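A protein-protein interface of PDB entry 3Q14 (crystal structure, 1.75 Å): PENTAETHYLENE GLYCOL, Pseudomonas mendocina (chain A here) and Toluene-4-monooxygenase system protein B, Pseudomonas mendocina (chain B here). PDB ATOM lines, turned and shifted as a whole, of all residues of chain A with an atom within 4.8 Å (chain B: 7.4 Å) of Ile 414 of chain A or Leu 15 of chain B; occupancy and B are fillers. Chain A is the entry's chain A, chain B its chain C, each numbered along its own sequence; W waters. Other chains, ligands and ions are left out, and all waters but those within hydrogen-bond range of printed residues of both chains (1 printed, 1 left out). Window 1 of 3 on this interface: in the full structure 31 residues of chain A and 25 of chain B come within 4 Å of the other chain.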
ATOM      1  N   TRP A 338     -14.810 -23.130  17.885  1.00  0.00           N
ATOM      2  CA  TRP A 338     -15.607 -24.032  18.720  1.00  0.00           C
ATOM      3  C   TRP A 338     -14.722 -24.847  19.676  1.00  0.00           C
ATOM      4  O   TRP A 338     -15.061 -25.970  20.047  1.00  0.00           O
ATOM      5  CB  TRP A 338     -16.470 -24.968  17.852  1.00  0.00           C
ATOM      6  CG  TRP A 338     -17.768 -24.342  17.385  1.00  0.00           C
ATOM      7  CD1 TRP A 338     -19.006 -24.508  17.938  1.00  0.00           C
ATOM      8  CD2 TRP A 338     -17.945 -23.467  16.264  1.00  0.00           C
ATOM      9  NE1 TRP A 338     -19.936 -23.767  17.250  1.00  0.00           N
ATOM     10  CE2 TRP A 338     -19.313 -23.127  16.211  1.00  0.00           C
ATOM     11  CE3 TRP A 338     -17.076 -22.927  15.309  1.00  0.00           C
ATOM     12  CZ2 TRP A 338     -19.833 -22.276  15.241  1.00  0.00           C
ATOM     13  CZ3 TRP A 338     -17.596 -22.085  14.338  1.00  0.00           C
ATOM     14  CH2 TRP A 338     -18.964 -21.766  14.313  1.00  0.00           C
ATOM     15  N   PRO A 394     -22.242 -25.568  14.223  1.00  0.00           N
ATOM     16  CA  PRO A 394     -21.881 -25.612  12.804  1.00  0.00           C
ATOM     17  C   PRO A 394     -22.702 -26.680  12.092  1.00  0.00           C
ATOM     18  O   PRO A 394     -23.144 -27.632  12.734  1.00  0.00           O
ATOM     19  CB  PRO A 394     -20.407 -26.028  12.834  1.00  0.00           C
ATOM     20  CG  PRO A 394     -20.248 -26.774  14.114  1.00  0.00           C
ATOM     21  CD  PRO A 394     -21.196 -26.137  15.092  1.00  0.00           C
ATOM     22  N   LEU A 404     -19.197 -28.244   7.728  1.00  0.00           N
ATOM     23  CA  LEU A 404     -19.196 -27.872   6.310  1.00  0.00           C
ATOM     24  C   LEU A 404     -18.500 -26.526   6.138  1.00  0.00           C
ATOM     25  O   LEU A 404     -18.981 -25.510   6.645  1.00  0.00           O
ATOM     26  CB  LEU A 404     -20.644 -27.765   5.814  1.00  0.00           C
ATOM     27  CG  LEU A 404     -21.476 -29.048   5.929  1.00  0.00           C
ATOM     28  CD1 LEU A 404     -22.957 -28.783   5.658  1.00  0.00           C
ATOM     29  CD2 LEU A 404     -20.930 -30.107   4.956  1.00  0.00           C
ATOM     30  N   VAL A 405     -17.377 -26.510   5.422  1.00  0.00           N
ATOM     31  CA  VAL A 405     -16.580 -25.288   5.312  1.00  0.00           C
ATOM     32  C   VAL A 405     -16.298 -24.906   3.866  1.00  0.00           C
ATOM     33  O   VAL A 405     -16.568 -25.672   2.937  1.00  0.00           O
ATOM     34  CB  VAL A 405     -15.220 -25.421   6.052  1.00  0.00           C
ATOM     35  CG1 VAL A 405     -15.438 -25.693   7.537  1.00  0.00           C
ATOM     36  CG2 VAL A 405     -14.369 -26.511   5.415  1.00  0.00           C
ATOM     37  N   GLY A 406     -15.739 -23.714   3.687  1.00  0.00           N
ATOM     38  CA  GLY A 406     -15.353 -23.231   2.377  1.00  0.00           C
ATOM     39  C   GLY A 406     -14.198 -22.265   2.528  1.00  0.00           C
ATOM     40  O   GLY A 406     -13.536 -22.252   3.561  1.00  0.00           O
ATOM     41  N   TRP A 412     -14.560 -15.456  -1.405  1.00  0.00           N
ATOM     42  CA  TRP A 412     -15.479 -16.365  -0.740  1.00  0.00           C
ATOM     43  C   TRP A 412     -16.076 -17.408  -1.679  1.00  0.00           C
ATOM     44  O   TRP A 412     -16.619 -17.079  -2.734  1.00  0.00           O
ATOM     45  CB  TRP A 412     -16.609 -15.550  -0.116  1.00  0.00           C
ATOM     46  CG  TRP A 412     -17.631 -16.354   0.618  1.00  0.00           C
ATOM     47  CD1 TRP A 412     -17.421 -17.153   1.704  1.00  0.00           C
ATOM     48  CD2 TRP A 412     -19.032 -16.419   0.337  1.00  0.00           C
ATOM     49  NE1 TRP A 412     -18.605 -17.714   2.113  1.00  0.00           N
ATOM     50  CE2 TRP A 412     -19.611 -17.276   1.294  1.00  0.00           C
ATOM     51  CE3 TRP A 412     -19.860 -15.829  -0.633  1.00  0.00           C
ATOM     52  CZ2 TRP A 412     -20.973 -17.568   1.310  1.00  0.00           C
ATOM     53  CZ3 TRP A 412     -21.214 -16.113  -0.610  1.00  0.00           C
ATOM     54  CH2 TRP A 412     -21.757 -16.976   0.352  1.00  0.00           C
ATOM     55  N   ASN A 413     -15.968 -18.672  -1.290  1.00  0.00           N
ATOM     56  CA  ASN A 413     -16.634 -19.740  -2.013  1.00  0.00           C
ATOM     57  C   ASN A 413     -16.883 -20.913  -1.090  1.00  0.00           C
ATOM     58  O   ASN A 413     -15.956 -21.456  -0.488  1.00  0.00           O
ATOM     59  CB  ASN A 413     -15.827 -20.187  -3.235  1.00  0.00           C
ATOM     60  CG  ASN A 413     -16.586 -21.199  -4.091  1.00  0.00           C
ATOM     61  OD1 ASN A 413     -17.475 -20.835  -4.860  1.00  0.00           O
ATOM     62  ND2 ASN A 413     -16.242 -22.475  -3.949  1.00  0.00           N
ATOM     63  N   ILE A 414     -18.147 -21.291  -0.967  1.00  0.00           N
ATOM     64  CA  ILE A 414     -18.498 -22.427  -0.141  1.00  0.00           C
ATOM     65  C   ILE A 414     -19.584 -23.233  -0.850  1.00  0.00           C
ATOM     66  O   ILE A 414     -20.513 -22.668  -1.432  1.00  0.00           O
ATOM     67  CB  ILE A 414     -18.910 -21.970   1.280  1.00  0.00           C
ATOM     68  CG1 ILE A 414     -19.112 -23.167   2.212  1.00  0.00           C
ATOM     69  CG2 ILE A 414     -20.138 -21.075   1.251  1.00  0.00           C
ATOM     70  CD1 ILE A 414     -19.087 -22.772   3.683  1.00  0.00           C
ATOM     71  N   GLU A 415     -19.428 -24.552  -0.847  1.00  0.00           N
ATOM     72  CA  GLU A 415     -20.408 -25.418  -1.479  1.00  0.00           C
ATOM     73  C   GLU A 415     -20.761 -26.626  -0.620  1.00  0.00           C
ATOM     74  O   GLU A 415     -19.887 -27.344  -0.130  1.00  0.00           O
ATOM     75  CB  GLU A 415     -19.943 -25.863  -2.866  1.00  0.00           C
ATOM     76  CG  GLU A 415     -21.041 -26.594  -3.628  1.00  0.00           C
ATOM     77  CD  GLU A 415     -20.769 -26.704  -5.118  1.00  0.00           C
ATOM     78  OE1 GLU A 415     -19.651 -26.350  -5.563  1.00  0.00           O
ATOM     79  OE2 GLU A 415     -21.689 -27.149  -5.841  1.00  0.00           O
ATOM     80  N   VAL A 416     -22.062 -26.819  -0.433  1.00  0.00           N
ATOM     81  CA  VAL A 416     -22.598 -27.995   0.228  1.00  0.00           C
ATOM     82  C   VAL A 416     -23.221 -28.870  -0.855  1.00  0.00           C
ATOM     83  O   VAL A 416     -23.898 -28.371  -1.757  1.00  0.00           O
ATOM     84  CB  VAL A 416     -23.689 -27.601   1.252  1.00  0.00           C
ATOM     85  CG1 VAL A 416     -24.279 -28.845   1.917  1.00  0.00           C
ATOM     86  CG2 VAL A 416     -23.111 -26.660   2.301  1.00  0.00           C
ATOM     87  N   ALA B   8     -27.148 -22.104   7.065  1.00  0.00           N
ATOM     88  CA  ALA B   8     -26.872 -20.846   6.381  1.00  0.00           C
ATOM     89  C   ALA B   8     -25.387 -20.554   6.206  1.00  0.00           C
ATOM     90  O   ALA B   8     -24.590 -20.674   7.147  1.00  0.00           O
ATOM     91  CB  ALA B   8     -27.554 -19.676   7.125  1.00  0.00           C
ATOM     92  N   ALA B   9     -25.033 -20.136   4.997  1.00  0.00           N
ATOM     93  CA  ALA B   9     -23.679 -19.699   4.687  1.00  0.00           C
ATOM     94  C   ALA B   9     -23.668 -18.190   4.482  1.00  0.00           C
ATOM     95  O   ALA B   9     -24.322 -17.681   3.566  1.00  0.00           O
ATOM     96  CB  ALA B   9     -23.181 -20.391   3.447  1.00  0.00           C
ATOM     97  N   PHE B  10     -22.934 -17.474   5.328  1.00  0.00           N
ATOM     98  CA  PHE B  10     -22.879 -16.020   5.220  1.00  0.00           C
ATOM     99  C   PHE B  10     -21.699 -15.587   4.352  1.00  0.00           C
ATOM    100  O   PHE B  10     -20.614 -16.168   4.428  1.00  0.00           O
ATOM    101  CB  PHE B  10     -22.804 -15.376   6.607  1.00  0.00           C
ATOM    102  CG  PHE B  10     -23.068 -13.903   6.595  1.00  0.00           C
ATOM    103  CD1 PHE B  10     -22.041 -13.006   6.373  1.00  0.00           C
ATOM    104  CD2 PHE B  10     -24.350 -13.418   6.779  1.00  0.00           C
ATOM    105  CE1 PHE B  10     -22.285 -11.641   6.352  1.00  0.00           C
ATOM    106  CE2 PHE B  10     -24.605 -12.056   6.758  1.00  0.00           C
ATOM    107  CZ  PHE B  10     -23.571 -11.166   6.541  1.00  0.00           C
ATOM    108  N   GLU B  11     -21.917 -14.565   3.528  1.00  0.00           N
ATOM    109  CA  GLU B  11     -20.910 -14.114   2.569  1.00  0.00           C
ATOM    110  C   GLU B  11     -19.591 -13.703   3.228  1.00  0.00           C
ATOM    111  O   GLU B  11     -19.568 -12.837   4.102  1.00  0.00           O
ATOM    112  CB  GLU B  11     -21.458 -12.957   1.725  1.00  0.00           C
ATOM    113  CG  GLU B  11     -20.463 -12.426   0.699  1.00  0.00           C
ATOM    114  CD  GLU B  11     -21.062 -11.359  -0.207  1.00  0.00           C
ATOM    115  OE1 GLU B  11     -22.301 -11.221  -0.235  1.00  0.00           O
ATOM    116  OE2 GLU B  11     -20.288 -10.655  -0.893  1.00  0.00           O
ATOM    117  N   LYS B  12     -18.507 -14.324   2.768  1.00  0.00           N
ATOM    118  CA  LYS B  12     -17.146 -14.121   3.285  1.00  0.00           C
ATOM    119  C   LYS B  12     -16.809 -14.890   4.571  1.00  0.00           C
ATOM    120  O   LYS B  12     -15.672 -14.832   5.044  1.00  0.00           O
ATOM    121  CB  LYS B  12     -16.808 -12.631   3.418  1.00  0.00           C
ATOM    122  CG  LYS B  12     -16.762 -11.919   2.073  1.00  0.00           C
ATOM    123  CD  LYS B  12     -16.207 -10.512   2.181  1.00  0.00           C
ATOM    124  CE  LYS B  12     -15.848  -9.983   0.798  1.00  0.00           C
ATOM    125  NZ  LYS B  12     -15.102  -8.696   0.864  1.00  0.00           N
ATOM    126  N   ASP B  13     -17.778 -15.607   5.136  1.00  0.00           N
ATOM    127  CA  ASP B  13     -17.500 -16.490   6.274  1.00  0.00           C
ATOM    128  C   ASP B  13     -16.859 -17.789   5.774  1.00  0.00           C
ATOM    129  O   ASP B  13     -16.749 -18.009   4.566  1.00  0.00           O
ATOM    130  CB  ASP B  13     -18.784 -16.789   7.047  1.00  0.00           C
ATOM    131  CG  ASP B  13     -18.529 -17.166   8.497  1.00  0.00           C
ATOM    132  OD1 ASP B  13     -17.354 -17.164   8.944  1.00  0.00           O
ATOM    133  OD2 ASP B  13     -19.525 -17.458   9.197  1.00  0.00           O
ATOM    134  N   PHE B  14     -16.442 -18.650   6.699  1.00  0.00           N
ATOM    135  CA  PHE B  14     -15.708 -19.856   6.325  1.00  0.00           C
ATOM    136  C   PHE B  14     -16.533 -21.128   6.447  1.00  0.00           C
ATOM    137  O   PHE B  14     -16.066 -22.205   6.080  1.00  0.00           O
ATOM    138  CB  PHE B  14     -14.445 -20.004   7.182  1.00  0.00           C
ATOM    139  CG  PHE B  14     -14.696 -20.626   8.529  1.00  0.00           C
ATOM    140  CD1 PHE B  14     -14.476 -21.984   8.734  1.00  0.00           C
ATOM    141  CD2 PHE B  14     -15.144 -19.855   9.590  1.00  0.00           C
ATOM    142  CE1 PHE B  14     -14.704 -22.562   9.971  1.00  0.00           C
ATOM    143  CE2 PHE B  14     -15.376 -20.429  10.831  1.00  0.00           C
ATOM    144  CZ  PHE B  14     -15.153 -21.781  11.023  1.00  0.00           C
ATOM    145  N   LEU B  15     -17.753 -21.021   6.966  1.00  0.00           N
ATOM    146  CA  LEU B  15     -18.544 -22.232   7.169  1.00  0.00           C
ATOM    147  C   LEU B  15     -20.042 -22.050   6.994  1.00  0.00           C
ATOM    148  O   LEU B  15     -20.534 -20.938   6.747  1.00  0.00           O
ATOM    149  CB  LEU B  15     -18.249 -22.843   8.550  1.00  0.00           C
ATOM    150  CG  LEU B  15     -19.085 -22.324   9.725  1.00  0.00           C
ATOM    151  CD1 LEU B  15     -18.740 -23.089  10.996  1.00  0.00           C
ATOM    152  CD2 LEU B  15     -18.877 -20.837   9.926  1.00  0.00           C
ATOM    153  N   VAL B  16     -20.756 -23.170   7.104  1.00  0.00           N
ATOM    154  CA  VAL B  16     -22.212 -23.182   7.117  1.00  0.00           C
ATOM    155  C   VAL B  16     -22.644 -23.488   8.542  1.00  0.00           C
ATOM    156  O   VAL B  16     -22.076 -24.358   9.194  1.00  0.00           O
ATOM    157  CB  VAL B  16     -22.790 -24.265   6.160  1.00  0.00           C
ATOM    158  CG1 VAL B  16     -24.313 -24.188   6.113  1.00  0.00           C
ATOM    159  CG2 VAL B  16     -22.186 -24.125   4.768  1.00  0.00           C
ATOM    160  N   GLN B  17     -23.637 -22.761   9.043  1.00  0.00           N
ATOM    161  CA  GLN B  17     -24.074 -22.959  10.423  1.00  0.00           C
ATOM    162  C   GLN B  17     -25.547 -23.275  10.518  1.00  0.00           C
ATOM    163  O   GLN B  17     -26.334 -22.897   9.652  1.00  0.00           O
ATOM    164  CB  GLN B  17     -23.821 -21.699  11.253  1.00  0.00           C
ATOM    165  CG  GLN B  17     -22.365 -21.377  11.436  1.00  0.00           C
ATOM    166  CD  GLN B  17     -22.179 -20.050  12.127  1.00  0.00           C
ATOM    167  OE1 GLN B  17     -22.564 -19.004  11.598  1.00  0.00           O
ATOM    168  NE2 GLN B  17     -21.613 -20.081  13.323  1.00  0.00           N
ATOM    169  N   LEU B  18     -25.916 -23.946  11.602  1.00  0.00           N
ATOM    170  CA  LEU B  18     -27.315 -24.139  11.928  1.00  0.00           C
ATOM    171  C   LEU B  18     -27.870 -22.840  12.494  1.00  0.00           C
ATOM    172  O   LEU B  18     -27.336 -22.295  13.462  1.00  0.00           O
ATOM    173  CB  LEU B  18     -27.477 -25.260  12.953  1.00  0.00           C
ATOM    174  CG  LEU B  18     -28.880 -25.374  13.551  1.00  0.00           C
ATOM    175  CD1 LEU B  18     -29.880 -25.829  12.486  1.00  0.00           C
ATOM    176  CD2 LEU B  18     -28.880 -26.325  14.740  1.00  0.00           C
ATOM    177  N   HIS B  37     -24.611 -14.450  13.852  1.00  0.00           N
ATOM    178  CA  HIS B  37     -23.626 -15.474  14.162  1.00  0.00           C
ATOM    179  C   HIS B  37     -22.362 -15.348  13.308  1.00  0.00           C
ATOM    180  O   HIS B  37     -21.516 -16.239  13.335  1.00  0.00           O
ATOM    181  CB  HIS B  37     -24.244 -16.868  13.994  1.00  0.00           C
ATOM    182  CG  HIS B  37     -25.386 -17.143  14.925  1.00  0.00           C
ATOM    183  ND1 HIS B  37     -25.202 -17.453  16.256  1.00  0.00           N
ATOM    184  CD2 HIS B  37     -26.725 -17.156  14.718  1.00  0.00           C
ATOM    185  CE1 HIS B  37     -26.377 -17.642  16.829  1.00  0.00           C
ATOM    186  NE2 HIS B  37     -27.318 -17.468  15.919  1.00  0.00           N
ATOM    187  N   CYS B  38     -22.234 -14.249  12.563  1.00  0.00           N
ATOM    188  CA  CYS B  38     -21.136 -14.097  11.601  1.00  0.00           C
ATOM    189  C   CYS B  38     -20.462 -12.727  11.623  1.00  0.00           C
ATOM    190  O   CYS B  38     -19.241 -12.625  11.784  1.00  0.00           O
ATOM    191  CB  CYS B  38     -21.633 -14.387  10.185  1.00  0.00           C
ATOM    192  SG  CYS B  38     -22.541 -15.932  10.061  1.00  0.00           S
ATOM    193  N   ARG B  42     -16.464 -13.255  12.560  1.00  0.00           N
ATOM    194  CA  ARG B  42     -15.481 -13.704  11.587  1.00  0.00           C
ATOM    195  C   ARG B  42     -15.586 -12.903  10.298  1.00  0.00           C
ATOM    196  O   ARG B  42     -14.753 -13.046   9.403  1.00  0.00           O
ATOM    197  CB  ARG B  42     -15.650 -15.202  11.310  1.00  0.00           C
ATOM    198  CG  ARG B  42     -15.444 -16.071  12.540  1.00  0.00           C
ATOM    199  CD  ARG B  42     -15.765 -17.522  12.253  1.00  0.00           C
ATOM    200  NE  ARG B  42     -17.122 -17.658  11.740  1.00  0.00           N
ATOM    201  CZ  ARG B  42     -18.203 -17.757  12.507  1.00  0.00           C
ATOM    202  NH1 ARG B  42     -19.401 -17.864  11.954  1.00  0.00           N
ATOM    203  NH2 ARG B  42     -18.087 -17.743  13.830  1.00  0.00           N
ATOM    204  N   ARG B  53     -30.816 -16.271  -0.555  1.00  0.00           N
ATOM    205  CA  ARG B  53     -31.087 -17.113  -1.715  1.00  0.00           C
ATOM    206  C   ARG B  53     -30.900 -18.571  -1.315  1.00  0.00           C
ATOM    207  O   ARG B  53     -30.184 -18.867  -0.360  1.00  0.00           O
ATOM    208  CB  ARG B  53     -30.128 -16.768  -2.857  1.00  0.00           C
ATOM    209  CG  ARG B  53     -28.673 -16.977  -2.472  1.00  0.00           C
ATOM    210  CD  ARG B  53     -27.722 -16.716  -3.622  1.00  0.00           C
ATOM    211  NE  ARG B  53     -26.374 -17.139  -3.253  1.00  0.00           N
ATOM    212  CZ  ARG B  53     -25.263 -16.632  -3.771  1.00  0.00           C
ATOM    213  NH1 ARG B  53     -24.081 -17.074  -3.360  1.00  0.00           N
ATOM    214  NH2 ARG B  53     -25.334 -15.676  -4.687  1.00  0.00           N
ATOM    215  N   HIS B  55     -29.089 -21.979  -1.501  1.00  0.00           N
ATOM    216  CA  HIS B  55     -27.659 -22.205  -1.703  1.00  0.00           C
ATOM    217  C   HIS B  55     -27.245 -22.339  -3.168  1.00  0.00           C
ATOM    218  O   HIS B  55     -27.764 -23.190  -3.897  1.00  0.00           O
ATOM    219  CB  HIS B  55     -27.222 -23.453  -0.940  1.00  0.00           C
ATOM    220  CG  HIS B  55     -25.738 -23.663  -0.909  1.00  0.00           C
ATOM    221  ND1 HIS B  55     -25.144 -24.841  -1.309  1.00  0.00           N
ATOM    222  CD2 HIS B  55     -24.731 -22.850  -0.512  1.00  0.00           C
ATOM    223  CE1 HIS B  55     -23.834 -24.744  -1.161  1.00  0.00           C
ATOM    224  NE2 HIS B  55     -23.557 -23.545  -0.683  1.00  0.00           N
ATOM    225  N   ARG B  56     -26.290 -21.505  -3.578  1.00  0.00           N
ATOM    226  CA  ARG B  56     -25.702 -21.555  -4.919  1.00  0.00           C
ATOM    227  C   ARG B  56     -26.673 -21.121  -6.018  1.00  0.00           C
ATOM    228  O   ARG B  56     -26.330 -21.159  -7.202  1.00  0.00           O
ATOM    229  CB  ARG B  56     -25.150 -22.952  -5.244  1.00  0.00           C
ATOM    230  CG  ARG B  56     -24.192 -23.540  -4.210  1.00  0.00           C
ATOM    231  CD  ARG B  56     -22.849 -22.812  -4.144  1.00  0.00           C
ATOM    232  NE  ARG B  56     -21.981 -23.087  -5.288  1.00  0.00           N
ATOM    233  CZ  ARG B  56     -20.712 -22.691  -5.368  1.00  0.00           C
ATOM    234  NH1 ARG B  56     -20.161 -22.015  -4.368  1.00  0.00           N
ATOM    235  NH2 ARG B  56     -19.988 -22.977  -6.443  1.00  0.00           N
ATOM    236  N   ILE B  78     -29.247 -22.234   2.806  1.00  0.00           N
ATOM    237  CA  ILE B  78     -29.369 -20.914   2.190  1.00  0.00           C
ATOM    238  C   ILE B  78     -28.055 -20.138   2.285  1.00  0.00           C
ATOM    239  O   ILE B  78     -27.203 -20.431   3.136  1.00  0.00           O
ATOM    240  CB  ILE B  78     -30.476 -20.065   2.854  1.00  0.00           C
ATOM    241  CG1 ILE B  78     -30.160 -19.853   4.335  1.00  0.00           C
ATOM    242  CG2 ILE B  78     -31.837 -20.714   2.667  1.00  0.00           C
ATOM    243  CD1 ILE B  78     -31.216 -19.014   5.067  1.00  0.00           C
ATOM    244  N   ASP B  79     -27.884 -19.167   1.395  1.00  0.00           N
ATOM    245  CA  ASP B  79     -26.776 -18.229   1.476  1.00  0.00           C
ATOM    246  C   ASP B  79     -27.334 -16.881   1.891  1.00  0.00           C
ATOM    247  O   ASP B  79     -28.460 -16.542   1.536  1.00  0.00           O
ATOM    248  CB  ASP B  79     -26.095 -18.056   0.114  1.00  0.00           C
ATOM    249  CG  ASP B  79     -25.551 -19.357  -0.446  1.00  0.00           C
ATOM    250  OD1 ASP B  79     -25.206 -20.257   0.350  1.00  0.00           O
ATOM    251  OD2 ASP B  79     -25.466 -19.473  -1.688  1.00  0.00           O
HETATM  252  O   HOH W   1     -22.380 -20.104  -1.748  1.00  0.00           O
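The backbone carbonyl oxygen of Leu 404 of chain A sits at hydrogen-bond distance from the backbone NH of Val 16 of chain B (3.0 Å). The backbone carbonyl oxygen (O) of Phe 14 of chain B lies within hydrogen-bond range of the backbone NH (N) of Gly 406 of chain A, 2.8 Å away. The indole nitrogen (NE1) of Trp 412 of chain A lies within hydrogen-bond range of the backbone carbonyl oxygen (O) of Phe 10 of chain B, at 3.4 Å. The indole nitrogen (NE1) of Trp 412 of chain A lies close to the backbone carbonyl oxygen (O) of Asp 13 of chain B (3.1 Å). The guanidinium group of Arg 56 of chain B is in hydrogen-bond range of the side-chain amide oxygen of Asn 413 of chain A (3.0 Å). NE2 of His 55 of chain B sits at hydrogen-bond distance from O of Ile 414 of chain A, 3.3 Å away. The backbone carbonyl oxygen of Ile 414 of chain A sits at hydrogen-bond distance from the guanidinium group of Arg 56 of chain B (3.0 Å). The side-chain carboxylate (OE1) of Glu 415 of chain A lies within salt-bridge range of the guanidinium group (NH2) of Arg 56 of chain B (3.5 Å). The indole nitrogen (NE1) of Trp 412 of chain A lies close to the backbone NH (N) of Lys 12 of chain B, 3.5 Å away.
N of Ala 9 of chain B lies within hydrogen-bond range of O of Ile 78 of chain B (2.9 Å). The side-chain sulfur of Cys 38 of chain B lies within hydrogen-bond range of the side-chain carboxylate of Asp 13 of chain B. The side-chain amide oxygen of Gln 17 of chain B sits close to the backbone carbonyl oxygen of His 37 of chain B, 3.4 Å away. The side-chain sulfur of Cys 38 of chain B is in hydrogen-bond range of the side-chain amide oxygen of Gln 17 of chain B, 3.4 Å away. The side-chain amide oxygen (OE1) of Gln 17 of chain B is in hydrogen-bond range of the guanidinium group (NH1) of Arg 42 of chain B (3.4 Å). The side-chain carboxylate (OD2) of Asp 79 of chain B sits at hydrogen-bond distance from the backbone NH (N) of Arg 56 of chain B (2.9 Å).
Leu 15 of chain B touches Trp 338 of chain A (CD1 to CH2, 3.6 Å). Pro 394 of chain A touches Leu 15 of chain B. Pro 394 of chain A touches Val 16 of chain B. Leu 404 of chain A touches Leu 15 of chain B (O to CA, 3.3 Å). O of Phe 14 of chain B touches CA of Val 405 of chain A, 3.2 Å away. CE2 of Trp 412 of chain A touches CA of Glu 11 of chain B (3.6 Å). Ile 414 of chain A touches Ala 9 of chain B (CG2 to CB, 3.8 Å). O of Phe 14 of chain B touches CD1 of Ile 414 of chain A, at 3.9 Å. Ile 414 of chain A touches Val 16 of chain B. Val 16 of chain B touches Val 416 of chain A (CG2 to CG2, 3.7 Å).
Of the printed residues of chain A, Leu 15 of chain B touches Trp 338 (3.6 Å), Pro 394 (3.8 Å), Leu 404 (3.3 Å) and Ile 414 (3.5 Å). Of the printed residues of chain B, Leu 404 of chain A touches Leu 15 and Val 16. Of the printed residues of chain A, Phe 14 of chain B touches Val 405 (3.2 Å), Gly 406 (2.8 Å) and Ile 414 (3.9 Å). Arg 53 of chain B touches none of the printed residues of chain A. Leu 18 of chain B touches none of the printed residues of chain A. The nearest residue of chain B that does not touch Ile 414 of chain A is Asp 79 of chain B (5.2 Å). The nearest residue of chain A that does not touch Leu 15 of chain B is Val 405 of chain A (4.1 Å).
Hydrophobic or aromatic side chains of chain A that line the printed part of chain B: Trp 338, Pro 394, Val 405, Trp 412, Ile 414 and Val 416. Of the 19 printed residues of chain B, 11 touch a printed residue of chain A. Hydrophobic or aromatic side chains of chain B that line the printed part of chain A: Ala 9, Leu 15, Val 16 and His 55.
Water W1 lies within hydrogen-bond range of the side-chain carboxylate of Asp 79 of chain B (3.2 Å) and the backbone carbonyl oxygen of Ile 414 of chain A (3.2 Å).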
